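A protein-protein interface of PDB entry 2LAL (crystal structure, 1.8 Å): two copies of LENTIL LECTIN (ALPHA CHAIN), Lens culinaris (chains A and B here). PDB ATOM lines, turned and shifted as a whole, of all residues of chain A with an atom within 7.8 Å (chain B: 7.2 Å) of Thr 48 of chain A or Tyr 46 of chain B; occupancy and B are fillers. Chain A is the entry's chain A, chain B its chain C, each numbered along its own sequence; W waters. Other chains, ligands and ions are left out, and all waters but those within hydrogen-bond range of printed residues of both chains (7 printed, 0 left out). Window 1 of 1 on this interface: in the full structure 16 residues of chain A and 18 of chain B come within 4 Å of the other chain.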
ATOM      1  N   GLU A   2       6.192  13.253  21.310  1.00  0.00           N
ATOM      2  CA  GLU A   2       7.418  12.474  21.171  1.00  0.00           C
ATOM      3  C   GLU A   2       7.664  12.133  19.703  1.00  0.00           C
ATOM      4  O   GLU A   2       6.855  11.556  19.042  1.00  0.00           O
ATOM      5  CB  GLU A   2       7.373  11.186  21.957  1.00  0.00           C
ATOM      6  CG  GLU A   2       6.654  11.211  23.232  1.00  0.00           C
ATOM      7  CD  GLU A   2       7.199  10.064  24.107  1.00  0.00           C
ATOM      8  OE1 GLU A   2       8.251   9.431  23.815  1.00  0.00           O
ATOM      9  OE2 GLU A   2       6.523   9.889  25.118  1.00  0.00           O
ATOM     10  N   THR A   3       8.880  12.299  19.300  1.00  0.00           N
ATOM     11  CA  THR A   3       9.193  11.534  18.076  1.00  0.00           C
ATOM     12  C   THR A   3      10.446  10.714  18.296  1.00  0.00           C
ATOM     13  O   THR A   3      11.178  10.812  19.283  1.00  0.00           O
ATOM     14  CB  THR A   3       9.395  12.510  16.938  1.00  0.00           C
ATOM     15  OG1 THR A   3      10.685  13.111  17.052  1.00  0.00           O
ATOM     16  CG2 THR A   3       8.344  13.563  16.964  1.00  0.00           C
ATOM     17  N   THR A   4      10.694   9.834  17.376  1.00  0.00           N
ATOM     18  CA  THR A   4      11.904   8.989  17.374  1.00  0.00           C
ATOM     19  C   THR A   4      12.233   8.645  15.912  1.00  0.00           C
ATOM     20  O   THR A   4      11.305   8.322  15.190  1.00  0.00           O
ATOM     21  CB  THR A   4      11.611   7.667  18.090  1.00  0.00           C
ATOM     22  OG1 THR A   4      12.531   7.429  19.142  1.00  0.00           O
ATOM     23  CG2 THR A   4      11.762   6.552  17.081  1.00  0.00           C
ATOM     24  N   SER A   5      13.486   8.590  15.655  1.00  0.00           N
ATOM     25  CA  SER A   5      13.906   8.321  14.259  1.00  0.00           C
ATOM     26  C   SER A   5      15.281   7.718  14.231  1.00  0.00           C
ATOM     27  O   SER A   5      16.101   7.824  15.149  1.00  0.00           O
ATOM     28  CB  SER A   5      13.726   9.542  13.420  1.00  0.00           C
ATOM     29  OG  SER A   5      14.637   9.744  12.413  1.00  0.00           O
ATOM     30  N   PHE A   6      15.576   6.803  13.326  1.00  0.00           N
ATOM     31  CA  PHE A   6      16.893   6.186  13.174  1.00  0.00           C
ATOM     32  C   PHE A   6      17.029   5.526  11.806  1.00  0.00           C
ATOM     33  O   PHE A   6      16.062   5.333  11.097  1.00  0.00           O
ATOM     34  CB  PHE A   6      17.210   5.210  14.280  1.00  0.00           C
ATOM     35  CG  PHE A   6      16.587   3.826  14.089  1.00  0.00           C
ATOM     36  CD1 PHE A   6      17.077   2.968  13.120  1.00  0.00           C
ATOM     37  CD2 PHE A   6      15.516   3.445  14.896  1.00  0.00           C
ATOM     38  CE1 PHE A   6      16.463   1.719  13.007  1.00  0.00           C
ATOM     39  CE2 PHE A   6      14.883   2.199  14.774  1.00  0.00           C
ATOM     40  CZ  PHE A   6      15.401   1.339  13.795  1.00  0.00           C
ATOM     41  N   ASN A  17      23.107  -0.686  19.737  1.00  0.00           N
ATOM     42  CA  ASN A  17      21.695  -0.288  19.908  1.00  0.00           C
ATOM     43  C   ASN A  17      20.747  -1.338  19.352  1.00  0.00           C
ATOM     44  O   ASN A  17      19.556  -1.067  19.092  1.00  0.00           O
ATOM     45  CB  ASN A  17      21.451   1.047  19.236  1.00  0.00           C
ATOM     46  CG  ASN A  17      21.998   0.949  17.816  1.00  0.00           C
ATOM     47  OD1 ASN A  17      22.485  -0.140  17.400  1.00  0.00           O
ATOM     48  ND2 ASN A  17      21.964   2.026  17.051  1.00  0.00           N
ATOM     49  N   LEU A  18      21.141  -2.574  19.177  1.00  0.00           N
ATOM     50  CA  LEU A  18      20.268  -3.721  18.923  1.00  0.00           C
ATOM     51  C   LEU A  18      20.375  -4.748  20.043  1.00  0.00           C
ATOM     52  O   LEU A  18      21.399  -4.910  20.669  1.00  0.00           O
ATOM     53  CB  LEU A  18      20.628  -4.378  17.596  1.00  0.00           C
ATOM     54  CG  LEU A  18      19.920  -4.098  16.352  1.00  0.00           C
ATOM     55  CD1 LEU A  18      19.217  -2.816  16.067  1.00  0.00           C
ATOM     56  CD2 LEU A  18      20.473  -4.736  15.067  1.00  0.00           C
ATOM     57  N   ILE A  19      19.316  -5.492  20.287  1.00  0.00           N
ATOM     58  CA  ILE A  19      19.228  -6.701  21.121  1.00  0.00           C
ATOM     59  C   ILE A  19      19.113  -7.939  20.211  1.00  0.00           C
ATOM     60  O   ILE A  19      18.228  -8.029  19.383  1.00  0.00           O
ATOM     61  CB  ILE A  19      18.030  -6.647  22.050  1.00  0.00           C
ATOM     62  CG1 ILE A  19      18.138  -5.536  23.089  1.00  0.00           C
ATOM     63  CG2 ILE A  19      17.773  -7.979  22.738  1.00  0.00           C
ATOM     64  CD1 ILE A  19      16.823  -5.185  23.732  1.00  0.00           C
ATOM     65  N   LEU A  45      16.087  -6.923  18.007  1.00  0.00           N
ATOM     66  CA  LEU A  45      15.111  -5.845  18.329  1.00  0.00           C
ATOM     67  C   LEU A  45      15.890  -4.513  18.377  1.00  0.00           C
ATOM     68  O   LEU A  45      17.055  -4.474  18.736  1.00  0.00           O
ATOM     69  CB  LEU A  45      14.567  -6.095  19.745  1.00  0.00           C
ATOM     70  CG  LEU A  45      13.841  -7.426  19.705  1.00  0.00           C
ATOM     71  CD1 LEU A  45      14.612  -8.581  20.191  1.00  0.00           C
ATOM     72  CD2 LEU A  45      12.386  -7.446  19.730  1.00  0.00           C
ATOM     73  N   TYR A  46      15.271  -3.455  17.958  1.00  0.00           N
ATOM     74  CA  TYR A  46      15.840  -2.142  18.358  1.00  0.00           C
ATOM     75  C   TYR A  46      15.723  -1.954  19.854  1.00  0.00           C
ATOM     76  O   TYR A  46      14.811  -2.381  20.564  1.00  0.00           O
ATOM     77  CB  TYR A  46      15.110  -1.050  17.611  1.00  0.00           C
ATOM     78  CG  TYR A  46      15.783   0.297  17.678  1.00  0.00           C
ATOM     79  CD1 TYR A  46      16.986   0.583  17.074  1.00  0.00           C
ATOM     80  CD2 TYR A  46      15.087   1.264  18.404  1.00  0.00           C
ATOM     81  CE1 TYR A  46      17.527   1.894  17.154  1.00  0.00           C
ATOM     82  CE2 TYR A  46      15.608   2.535  18.488  1.00  0.00           C
ATOM     83  CZ  TYR A  46      16.810   2.852  17.886  1.00  0.00           C
ATOM     84  OH  TYR A  46      17.252   4.136  18.007  1.00  0.00           O
ATOM     85  N   SER A  47      16.812  -1.448  20.409  1.00  0.00           N
ATOM     86  CA  SER A  47      16.908  -1.469  21.862  1.00  0.00           C
ATOM     87  C   SER A  47      15.978  -0.475  22.520  1.00  0.00           C
ATOM     88  O   SER A  47      15.536  -0.811  23.656  1.00  0.00           O
ATOM     89  CB  SER A  47      18.317  -1.397  22.360  1.00  0.00           C
ATOM     90  OG  SER A  47      18.642  -0.353  23.213  1.00  0.00           O
ATOM     91  N   THR A  48      15.659   0.674  21.989  1.00  0.00           N
ATOM     92  CA  THR A  48      14.821   1.661  22.704  1.00  0.00           C
ATOM     93  C   THR A  48      13.343   1.266  22.625  1.00  0.00           C
ATOM     94  O   THR A  48      12.851   1.056  21.520  1.00  0.00           O
ATOM     95  CB  THR A  48      14.959   3.008  22.001  1.00  0.00           C
ATOM     96  OG1 THR A  48      16.118   3.042  21.210  1.00  0.00           O
ATOM     97  CG2 THR A  48      14.875   4.110  22.970  1.00  0.00           C
ATOM     98  N   PRO A  49      12.638   1.400  23.736  1.00  0.00           N
ATOM     99  CA  PRO A  49      11.169   1.248  23.701  1.00  0.00           C
ATOM    100  C   PRO A  49      10.550   2.423  22.967  1.00  0.00           C
ATOM    101  O   PRO A  49      11.072   3.489  23.245  1.00  0.00           O
ATOM    102  CB  PRO A  49      10.852   1.365  25.189  1.00  0.00           C
ATOM    103  CG  PRO A  49      12.100   0.889  25.913  1.00  0.00           C
ATOM    104  CD  PRO A  49      13.231   1.518  25.062  1.00  0.00           C
ATOM    105  N   ILE A  50       9.583   2.191  22.153  1.00  0.00           N
ATOM    106  CA  ILE A  50       8.853   3.229  21.393  1.00  0.00           C
ATOM    107  C   ILE A  50       7.527   3.530  22.102  1.00  0.00           C
ATOM    108  O   ILE A  50       6.908   2.562  22.539  1.00  0.00           O
ATOM    109  CB  ILE A  50       8.554   2.744  19.985  1.00  0.00           C
ATOM    110  CG1 ILE A  50       9.771   2.180  19.302  1.00  0.00           C
ATOM    111  CG2 ILE A  50       7.849   3.801  19.156  1.00  0.00           C
ATOM    112  CD1 ILE A  50      11.056   2.950  19.420  1.00  0.00           C
ATOM    113  N   HIS A  51       7.186   4.771  22.240  1.00  0.00           N
ATOM    114  CA  HIS A  51       5.825   5.141  22.704  1.00  0.00           C
ATOM    115  C   HIS A  51       4.874   5.185  21.518  1.00  0.00           C
ATOM    116  O   HIS A  51       4.841   6.110  20.699  1.00  0.00           O
ATOM    117  CB  HIS A  51       5.863   6.520  23.370  1.00  0.00           C
ATOM    118  CG  HIS A  51       4.871   6.730  24.496  1.00  0.00           C
ATOM    119  ND1 HIS A  51       4.806   7.853  25.314  1.00  0.00           N
ATOM    120  CD2 HIS A  51       3.846   5.885  24.906  1.00  0.00           C
ATOM    121  CE1 HIS A  51       3.750   7.679  26.210  1.00  0.00           C
ATOM    122  NE2 HIS A  51       3.151   6.458  25.986  1.00  0.00           N
ATOM    123  N   VAL A  90       7.715  -4.785  25.455  1.00  0.00           N
ATOM    124  CA  VAL A  90       9.122  -4.374  25.602  1.00  0.00           C
ATOM    125  C   VAL A  90       9.998  -5.529  26.002  1.00  0.00           C
ATOM    126  O   VAL A  90      11.172  -5.726  25.599  1.00  0.00           O
ATOM    127  CB  VAL A  90       9.189  -3.236  26.642  1.00  0.00           C
ATOM    128  CG1 VAL A  90      10.347  -3.261  27.523  1.00  0.00           C
ATOM    129  CG2 VAL A  90       8.858  -1.822  26.161  1.00  0.00           C
ATOM    130  N   THR B   4      20.335   8.989  14.292  1.00  0.00           N
ATOM    131  CA  THR B   4      19.424   8.828  15.448  1.00  0.00           C
ATOM    132  C   THR B   4      18.808  10.216  15.743  1.00  0.00           C
ATOM    133  O   THR B   4      19.672  11.098  15.770  1.00  0.00           O
ATOM    134  CB  THR B   4      20.221   8.418  16.674  1.00  0.00           C
ATOM    135  OG1 THR B   4      20.722   7.111  16.604  1.00  0.00           O
ATOM    136  CG2 THR B   4      19.411   8.592  17.914  1.00  0.00           C
ATOM    137  N   SER B   5      17.575  10.379  15.907  1.00  0.00           N
ATOM    138  CA  SER B   5      16.804  11.537  16.329  1.00  0.00           C
ATOM    139  C   SER B   5      15.704  11.145  17.313  1.00  0.00           C
ATOM    140  O   SER B   5      15.090  10.104  17.289  1.00  0.00           O
ATOM    141  CB  SER B   5      16.179  12.281  15.165  1.00  0.00           C
ATOM    142  OG  SER B   5      17.005  12.130  14.043  1.00  0.00           O
ATOM    143  N   PHE B   6      15.392  12.089  18.164  1.00  0.00           N
ATOM    144  CA  PHE B   6      14.330  12.011  19.178  1.00  0.00           C
ATOM    145  C   PHE B   6      14.015  13.414  19.695  1.00  0.00           C
ATOM    146  O   PHE B   6      14.829  14.322  19.515  1.00  0.00           O
ATOM    147  CB  PHE B   6      14.695  11.075  20.298  1.00  0.00           C
ATOM    148  CG  PHE B   6      15.596  11.659  21.373  1.00  0.00           C
ATOM    149  CD1 PHE B   6      15.094  12.645  22.219  1.00  0.00           C
ATOM    150  CD2 PHE B   6      16.888  11.167  21.498  1.00  0.00           C
ATOM    151  CE1 PHE B   6      15.926  13.129  23.214  1.00  0.00           C
ATOM    152  CE2 PHE B   6      17.714  11.659  22.521  1.00  0.00           C
ATOM    153  CZ  PHE B   6      17.214  12.651  23.344  1.00  0.00           C
ATOM    154  N   SER B   7      12.824  13.710  19.983  1.00  0.00           N
ATOM    155  CA  SER B   7      12.242  14.911  20.576  1.00  0.00           C
ATOM    156  C   SER B   7      11.195  14.512  21.614  1.00  0.00           C
ATOM    157  O   SER B   7      10.371  13.666  21.348  1.00  0.00           O
ATOM    158  CB  SER B   7      11.639  15.814  19.532  1.00  0.00           C
ATOM    159  OG  SER B   7      10.204  15.604  19.669  1.00  0.00           O
ATOM    160  N   ILE B   8      11.403  14.940  22.840  1.00  0.00           N
ATOM    161  CA  ILE B   8      10.340  14.919  23.853  1.00  0.00           C
ATOM    162  C   ILE B   8       9.950  16.319  24.268  1.00  0.00           C
ATOM    163  O   ILE B   8      10.745  17.051  24.822  1.00  0.00           O
ATOM    164  CB  ILE B   8      10.812  14.134  25.070  1.00  0.00           C
ATOM    165  CG1 ILE B   8      11.447  12.832  24.595  1.00  0.00           C
ATOM    166  CG2 ILE B   8       9.662  13.890  26.028  1.00  0.00           C
ATOM    167  CD1 ILE B   8      12.199  11.988  25.575  1.00  0.00           C
ATOM    168  N   GLN B  16       9.617   5.248  29.555  1.00  0.00           N
ATOM    169  CA  GLN B  16      10.424   4.031  29.554  1.00  0.00           C
ATOM    170  C   GLN B  16      11.643   4.169  28.659  1.00  0.00           C
ATOM    171  O   GLN B  16      12.511   3.301  28.819  1.00  0.00           O
ATOM    172  CB  GLN B  16       9.628   2.801  29.174  1.00  0.00           C
ATOM    173  CG  GLN B  16       8.298   2.723  29.943  1.00  0.00           C
ATOM    174  CD  GLN B  16       8.013   1.245  30.250  1.00  0.00           C
ATOM    175  OE1 GLN B  16       8.968   0.372  29.901  1.00  0.00           O
ATOM    176  NE2 GLN B  16       6.921   0.792  30.842  1.00  0.00           N
ATOM    177  N   ASN B  17      11.828   5.184  27.842  1.00  0.00           N
ATOM    178  CA  ASN B  17      13.106   5.381  27.128  1.00  0.00           C
ATOM    179  C   ASN B  17      14.070   6.270  27.887  1.00  0.00           C
ATOM    180  O   ASN B  17      15.095   6.739  27.301  1.00  0.00           O
ATOM    181  CB  ASN B  17      12.834   5.984  25.750  1.00  0.00           C
ATOM    182  CG  ASN B  17      11.937   7.217  25.887  1.00  0.00           C
ATOM    183  OD1 ASN B  17      11.528   7.661  27.047  1.00  0.00           O
ATOM    184  ND2 ASN B  17      11.562   7.828  24.784  1.00  0.00           N
ATOM    185  N   LEU B  18      13.933   6.600  29.131  1.00  0.00           N
ATOM    186  CA  LEU B  18      14.903   7.303  29.998  1.00  0.00           C
ATOM    187  C   LEU B  18      15.374   6.350  31.112  1.00  0.00           C
ATOM    188  O   LEU B  18      14.629   5.490  31.599  1.00  0.00           O
ATOM    189  CB  LEU B  18      14.205   8.500  30.643  1.00  0.00           C
ATOM    190  CG  LEU B  18      14.568   9.862  30.255  1.00  0.00           C
ATOM    191  CD1 LEU B  18      14.413  10.368  28.869  1.00  0.00           C
ATOM    192  CD2 LEU B  18      14.279  10.923  31.314  1.00  0.00           C
ATOM    193  N   ILE B  19      16.622   6.441  31.515  1.00  0.00           N
ATOM    194  CA  ILE B  19      17.185   5.837  32.758  1.00  0.00           C
ATOM    195  C   ILE B  19      17.279   6.926  33.832  1.00  0.00           C
ATOM    196  O   ILE B  19      17.789   8.036  33.589  1.00  0.00           O
ATOM    197  CB  ILE B  19      18.563   5.271  32.462  1.00  0.00           C
ATOM    198  CG1 ILE B  19      18.536   4.256  31.322  1.00  0.00           C
ATOM    199  CG2 ILE B  19      19.248   4.699  33.670  1.00  0.00           C
ATOM    200  CD1 ILE B  19      19.885   3.650  31.003  1.00  0.00           C
ATOM    201  N   ALA B  44      19.331  11.611  34.541  1.00  0.00           N
ATOM    202  CA  ALA B  44      18.508  11.012  33.489  1.00  0.00           C
ATOM    203  C   ALA B  44      19.313  10.856  32.200  1.00  0.00           C
ATOM    204  O   ALA B  44      19.771  11.861  31.652  1.00  0.00           O
ATOM    205  CB  ALA B  44      17.271  11.842  33.228  1.00  0.00           C
ATOM    206  N   LEU B  45      19.551   9.607  31.819  1.00  0.00           N
ATOM    207  CA  LEU B  45      20.184   9.208  30.543  1.00  0.00           C
ATOM    208  C   LEU B  45      19.054   8.799  29.559  1.00  0.00           C
ATOM    209  O   LEU B  45      18.050   8.247  29.954  1.00  0.00           O
ATOM    210  CB  LEU B  45      21.049   7.972  30.741  1.00  0.00           C
ATOM    211  CG  LEU B  45      21.791   7.999  32.101  1.00  0.00           C
ATOM    212  CD1 LEU B  45      22.606   6.710  32.140  1.00  0.00           C
ATOM    213  CD2 LEU B  45      22.707   9.204  32.055  1.00  0.00           C
ATOM    214  N   TYR B  46      19.278   9.187  28.367  1.00  0.00           N
ATOM    215  CA  TYR B  46      18.598   8.574  27.216  1.00  0.00           C
ATOM    216  C   TYR B  46      18.990   7.126  27.087  1.00  0.00           C
ATOM    217  O   TYR B  46      20.153   6.739  27.372  1.00  0.00           O
ATOM    218  CB  TYR B  46      18.931   9.372  25.963  1.00  0.00           C
ATOM    219  CG  TYR B  46      18.007   8.950  24.829  1.00  0.00           C
ATOM    220  CD1 TYR B  46      16.640   9.227  24.910  1.00  0.00           C
ATOM    221  CD2 TYR B  46      18.605   8.254  23.777  1.00  0.00           C
ATOM    222  CE1 TYR B  46      15.790   8.808  23.854  1.00  0.00           C
ATOM    223  CE2 TYR B  46      17.771   7.857  22.748  1.00  0.00           C
ATOM    224  CZ  TYR B  46      16.399   8.129  22.795  1.00  0.00           C
ATOM    225  OH  TYR B  46      15.636   7.684  21.732  1.00  0.00           O
ATOM    226  N   SER B  47      18.052   6.207  26.925  1.00  0.00           N
ATOM    227  CA  SER B  47      18.374   4.813  27.190  1.00  0.00           C
ATOM    228  C   SER B  47      19.272   4.208  26.135  1.00  0.00           C
ATOM    229  O   SER B  47      20.018   3.259  26.508  1.00  0.00           O
ATOM    230  CB  SER B  47      17.207   3.950  27.523  1.00  0.00           C
ATOM    231  OG  SER B  47      16.238   3.665  26.570  1.00  0.00           O
ATOM    232  N   THR B  48      19.245   4.707  24.923  1.00  0.00           N
ATOM    233  CA  THR B  48      19.864   4.002  23.778  1.00  0.00           C
ATOM    234  C   THR B  48      21.324   4.409  23.630  1.00  0.00           C
ATOM    235  O   THR B  48      21.529   5.637  23.601  1.00  0.00           O
ATOM    236  CB  THR B  48      19.124   4.434  22.500  1.00  0.00           C
ATOM    237  OG1 THR B  48      17.731   4.390  22.742  1.00  0.00           O
ATOM    238  CG2 THR B  48      19.484   3.499  21.389  1.00  0.00           C
ATOM    239  N   PRO B  49      22.198   3.425  23.404  1.00  0.00           N
ATOM    240  CA  PRO B  49      23.608   3.804  23.169  1.00  0.00           C
ATOM    241  C   PRO B  49      23.728   4.532  21.853  1.00  0.00           C
ATOM    242  O   PRO B  49      23.032   4.109  20.944  1.00  0.00           O
ATOM    243  CB  PRO B  49      24.273   2.450  23.115  1.00  0.00           C
ATOM    244  CG  PRO B  49      23.432   1.541  24.019  1.00  0.00           C
ATOM    245  CD  PRO B  49      22.004   1.984  23.563  1.00  0.00           C
ATOM    246  N   ILE B  50      24.451   5.632  21.900  1.00  0.00           N
ATOM    247  CA  ILE B  50      24.803   6.380  20.709  1.00  0.00           C
ATOM    248  C   ILE B  50      26.203   6.061  20.217  1.00  0.00           C
ATOM    249  O   ILE B  50      27.138   5.903  20.938  1.00  0.00           O
ATOM    250  CB  ILE B  50      24.600   7.870  20.861  1.00  0.00           C
ATOM    251  CG1 ILE B  50      23.116   8.209  20.995  1.00  0.00           C
ATOM    252  CG2 ILE B  50      25.172   8.607  19.631  1.00  0.00           C
ATOM    253  CD1 ILE B  50      22.340   8.135  22.202  1.00  0.00           C
ATOM    254  N   VAL B  90      28.609   3.836  28.346  1.00  0.00           N
ATOM    255  CA  VAL B  90      27.196   3.434  28.368  1.00  0.00           C
ATOM    256  C   VAL B  90      26.799   3.026  29.773  1.00  0.00           C
ATOM    257  O   VAL B  90      25.627   3.183  30.165  1.00  0.00           O
ATOM    258  CB  VAL B  90      26.894   2.307  27.379  1.00  0.00           C
ATOM    259  CG1 VAL B  90      26.860   2.490  25.888  1.00  0.00           C
ATOM    260  CG2 VAL B  90      27.167   0.931  27.848  1.00  0.00           C
HETATM  261  O   HOH W   1      13.165   8.504  21.512  1.00  0.00           O
HETATM  262  O   HOH W   2      16.430   6.105  19.538  1.00  0.00           O
HETATM  263  O   HOH W   3      12.016   6.108  21.885  1.00  0.00           O
HETATM  264  O   HOH W   4      19.569   4.521  16.880  1.00  0.00           O
HETATM  265  O   HOH W   5      21.605   4.758  18.678  1.00  0.00           O
HETATM  266  O   HOH W   6      11.382  10.381  21.972  1.00  0.00           O
HETATM  267  O   HOH W   7      17.454   9.493  12.288  1.00  0.00           O
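Thr 48 of chain A touches just these residues of chain B: Asn 17, Tyr 46, Ser 47 and Thr 48.
Of chain A, only Thr 48 comes within 4 Å of Tyr 46 of chain B.
Of the printed residues of chain A, Asn 17 of chain B touches Glu 2, Thr 48 and Pro 49.
Printed residues of chain A within 4 Å of Ser 47 of chain B: Thr 48 (3.9 Å) and Pro 49 (3.99 Å).
Of the printed residues of chain A, Ser 5 of chain B touches Thr 4 and Ser 5.
The nearest printed residue of chain A that does not touch Gln 16 of chain B is Val 90 of chain A (4.3 Å).
Water W4 lies within hydrogen-bond range of the side-chain hydroxyl (OH) of Tyr 46 of chain A, the side-chain hydroxyl (OG1) of Thr 4 of chain B and the side-chain amide nitrogen (ND2) of Asn 17 of chain A.
Water W1 lies within hydrogen-bond range of the side-chain hydroxyl of Tyr 46 of chain B (2.6 Å) and the side-chain hydroxyl of Thr 4 of chain A (2.7 Å).
Water W2 bridges OH of Tyr 46 of chain A (2.6 Å) and OH of Tyr 46 of chain B (2.8 Å).
Water W6 bridges the backbone carbonyl oxygen (O) of Thr 3 of chain A and the backbone carbonyl oxygen (O) of Ser 7 of chain B.
Water W7 lies within hydrogen-bond range of OG of Ser 5 of chain A, OG of Ser 5 of chain B and N of Phe 6 of chain A.
Water W3 lies within hydrogen-bond range of the side-chain hydroxyl of Thr 4 of chain A (3.1 Å), the backbone carbonyl oxygen of Pro 49 of chain A (3.1 Å) and the side-chain amide nitrogen of Asn 17 of chain B (3.4 Å).
ND2 of Asn 17 of chain B touches OE1 of Glu 2 of chain A, at 3.8 Å.
Phe 6 of chain B touches Thr 3 of chain A (CA to O, 3.4 Å).
CA of Thr 4 of chain A touches O of Ser 5 of chain B (3.4 Å).
Ser 5 of chain A touches Thr 4 of chain B (O to CA, 3.5 Å).
Pro 49 of chain B touches Asn 17 of chain A.
Thr 48 of chain A touches Asn 17 of chain B (CG2 to CB, 3.9 Å).
Thr 48 of chain A touches Tyr 46 of chain B.
Ser 47 of chain B touches Thr 48 of chain A.
Pro 49 of chain A touches Gln 16 of chain B (CG to O, 3.8 Å).
Pro 49 of chain A touches Ser 47 of chain B (CD to OG, 3.99 Å).
N of Thr 3 of chain A sits at hydrogen-bond distance from O of Ser 7 of chain B, at 2.9 Å.
The backbone NH (N) of Ser 5 of chain A sits at hydrogen-bond distance from the backbone carbonyl oxygen (O) of Ser 5 of chain B (2.7 Å).
The side-chain hydroxyl of Thr 48 of chain A is in hydrogen-bond range of the side-chain hydroxyl of Thr 48 of chain B (2.6 Å).
ND1 of His 51 of chain A is in hydrogen-bond range of OE2 of Glu 2 of chain A (2.7 Å).
The backbone NH (N) of Ser 47 of chain A lies within hydrogen-bond range of the backbone carbonyl oxygen (O) of Asn 17 of chain A (3.1 Å).
O of Asn 17 of chain B is in hydrogen-bond range of N of Ser 47 of chain B, at 3.0 Å.
Thr 4 of chain A touches Ser 5 of chain B, and with the chains exchanged Ser 5 of chain A touches Thr 4 of chain B.
Ser 5 of chain A touches its own counterpart, Ser 5 of chain B.
Thr 48 of chain A touches Tyr 46 of chain B, but with the chains exchanged Tyr 46 of chain A does not touch Thr 48 of chain B (4.1 Å).
Pro 49 of chain A touches Ser 47 of chain B, but with the chains exchanged Ser 47 of chain A does not touch Pro 49 of chain B (4.1 Å).
Along chain B the printed residues that touch a printed residue of chain A span positions 4 to 49.
Of the 16 printed residues of chain A, 7 touch a printed residue of chain B.
Among the printed residues, 16 pairs touch across the chains.
Among the printed residues, no Asp or Glu carboxylate lies within 4 Å of a Lys or Arg side-chain nitrogen of the other chain.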
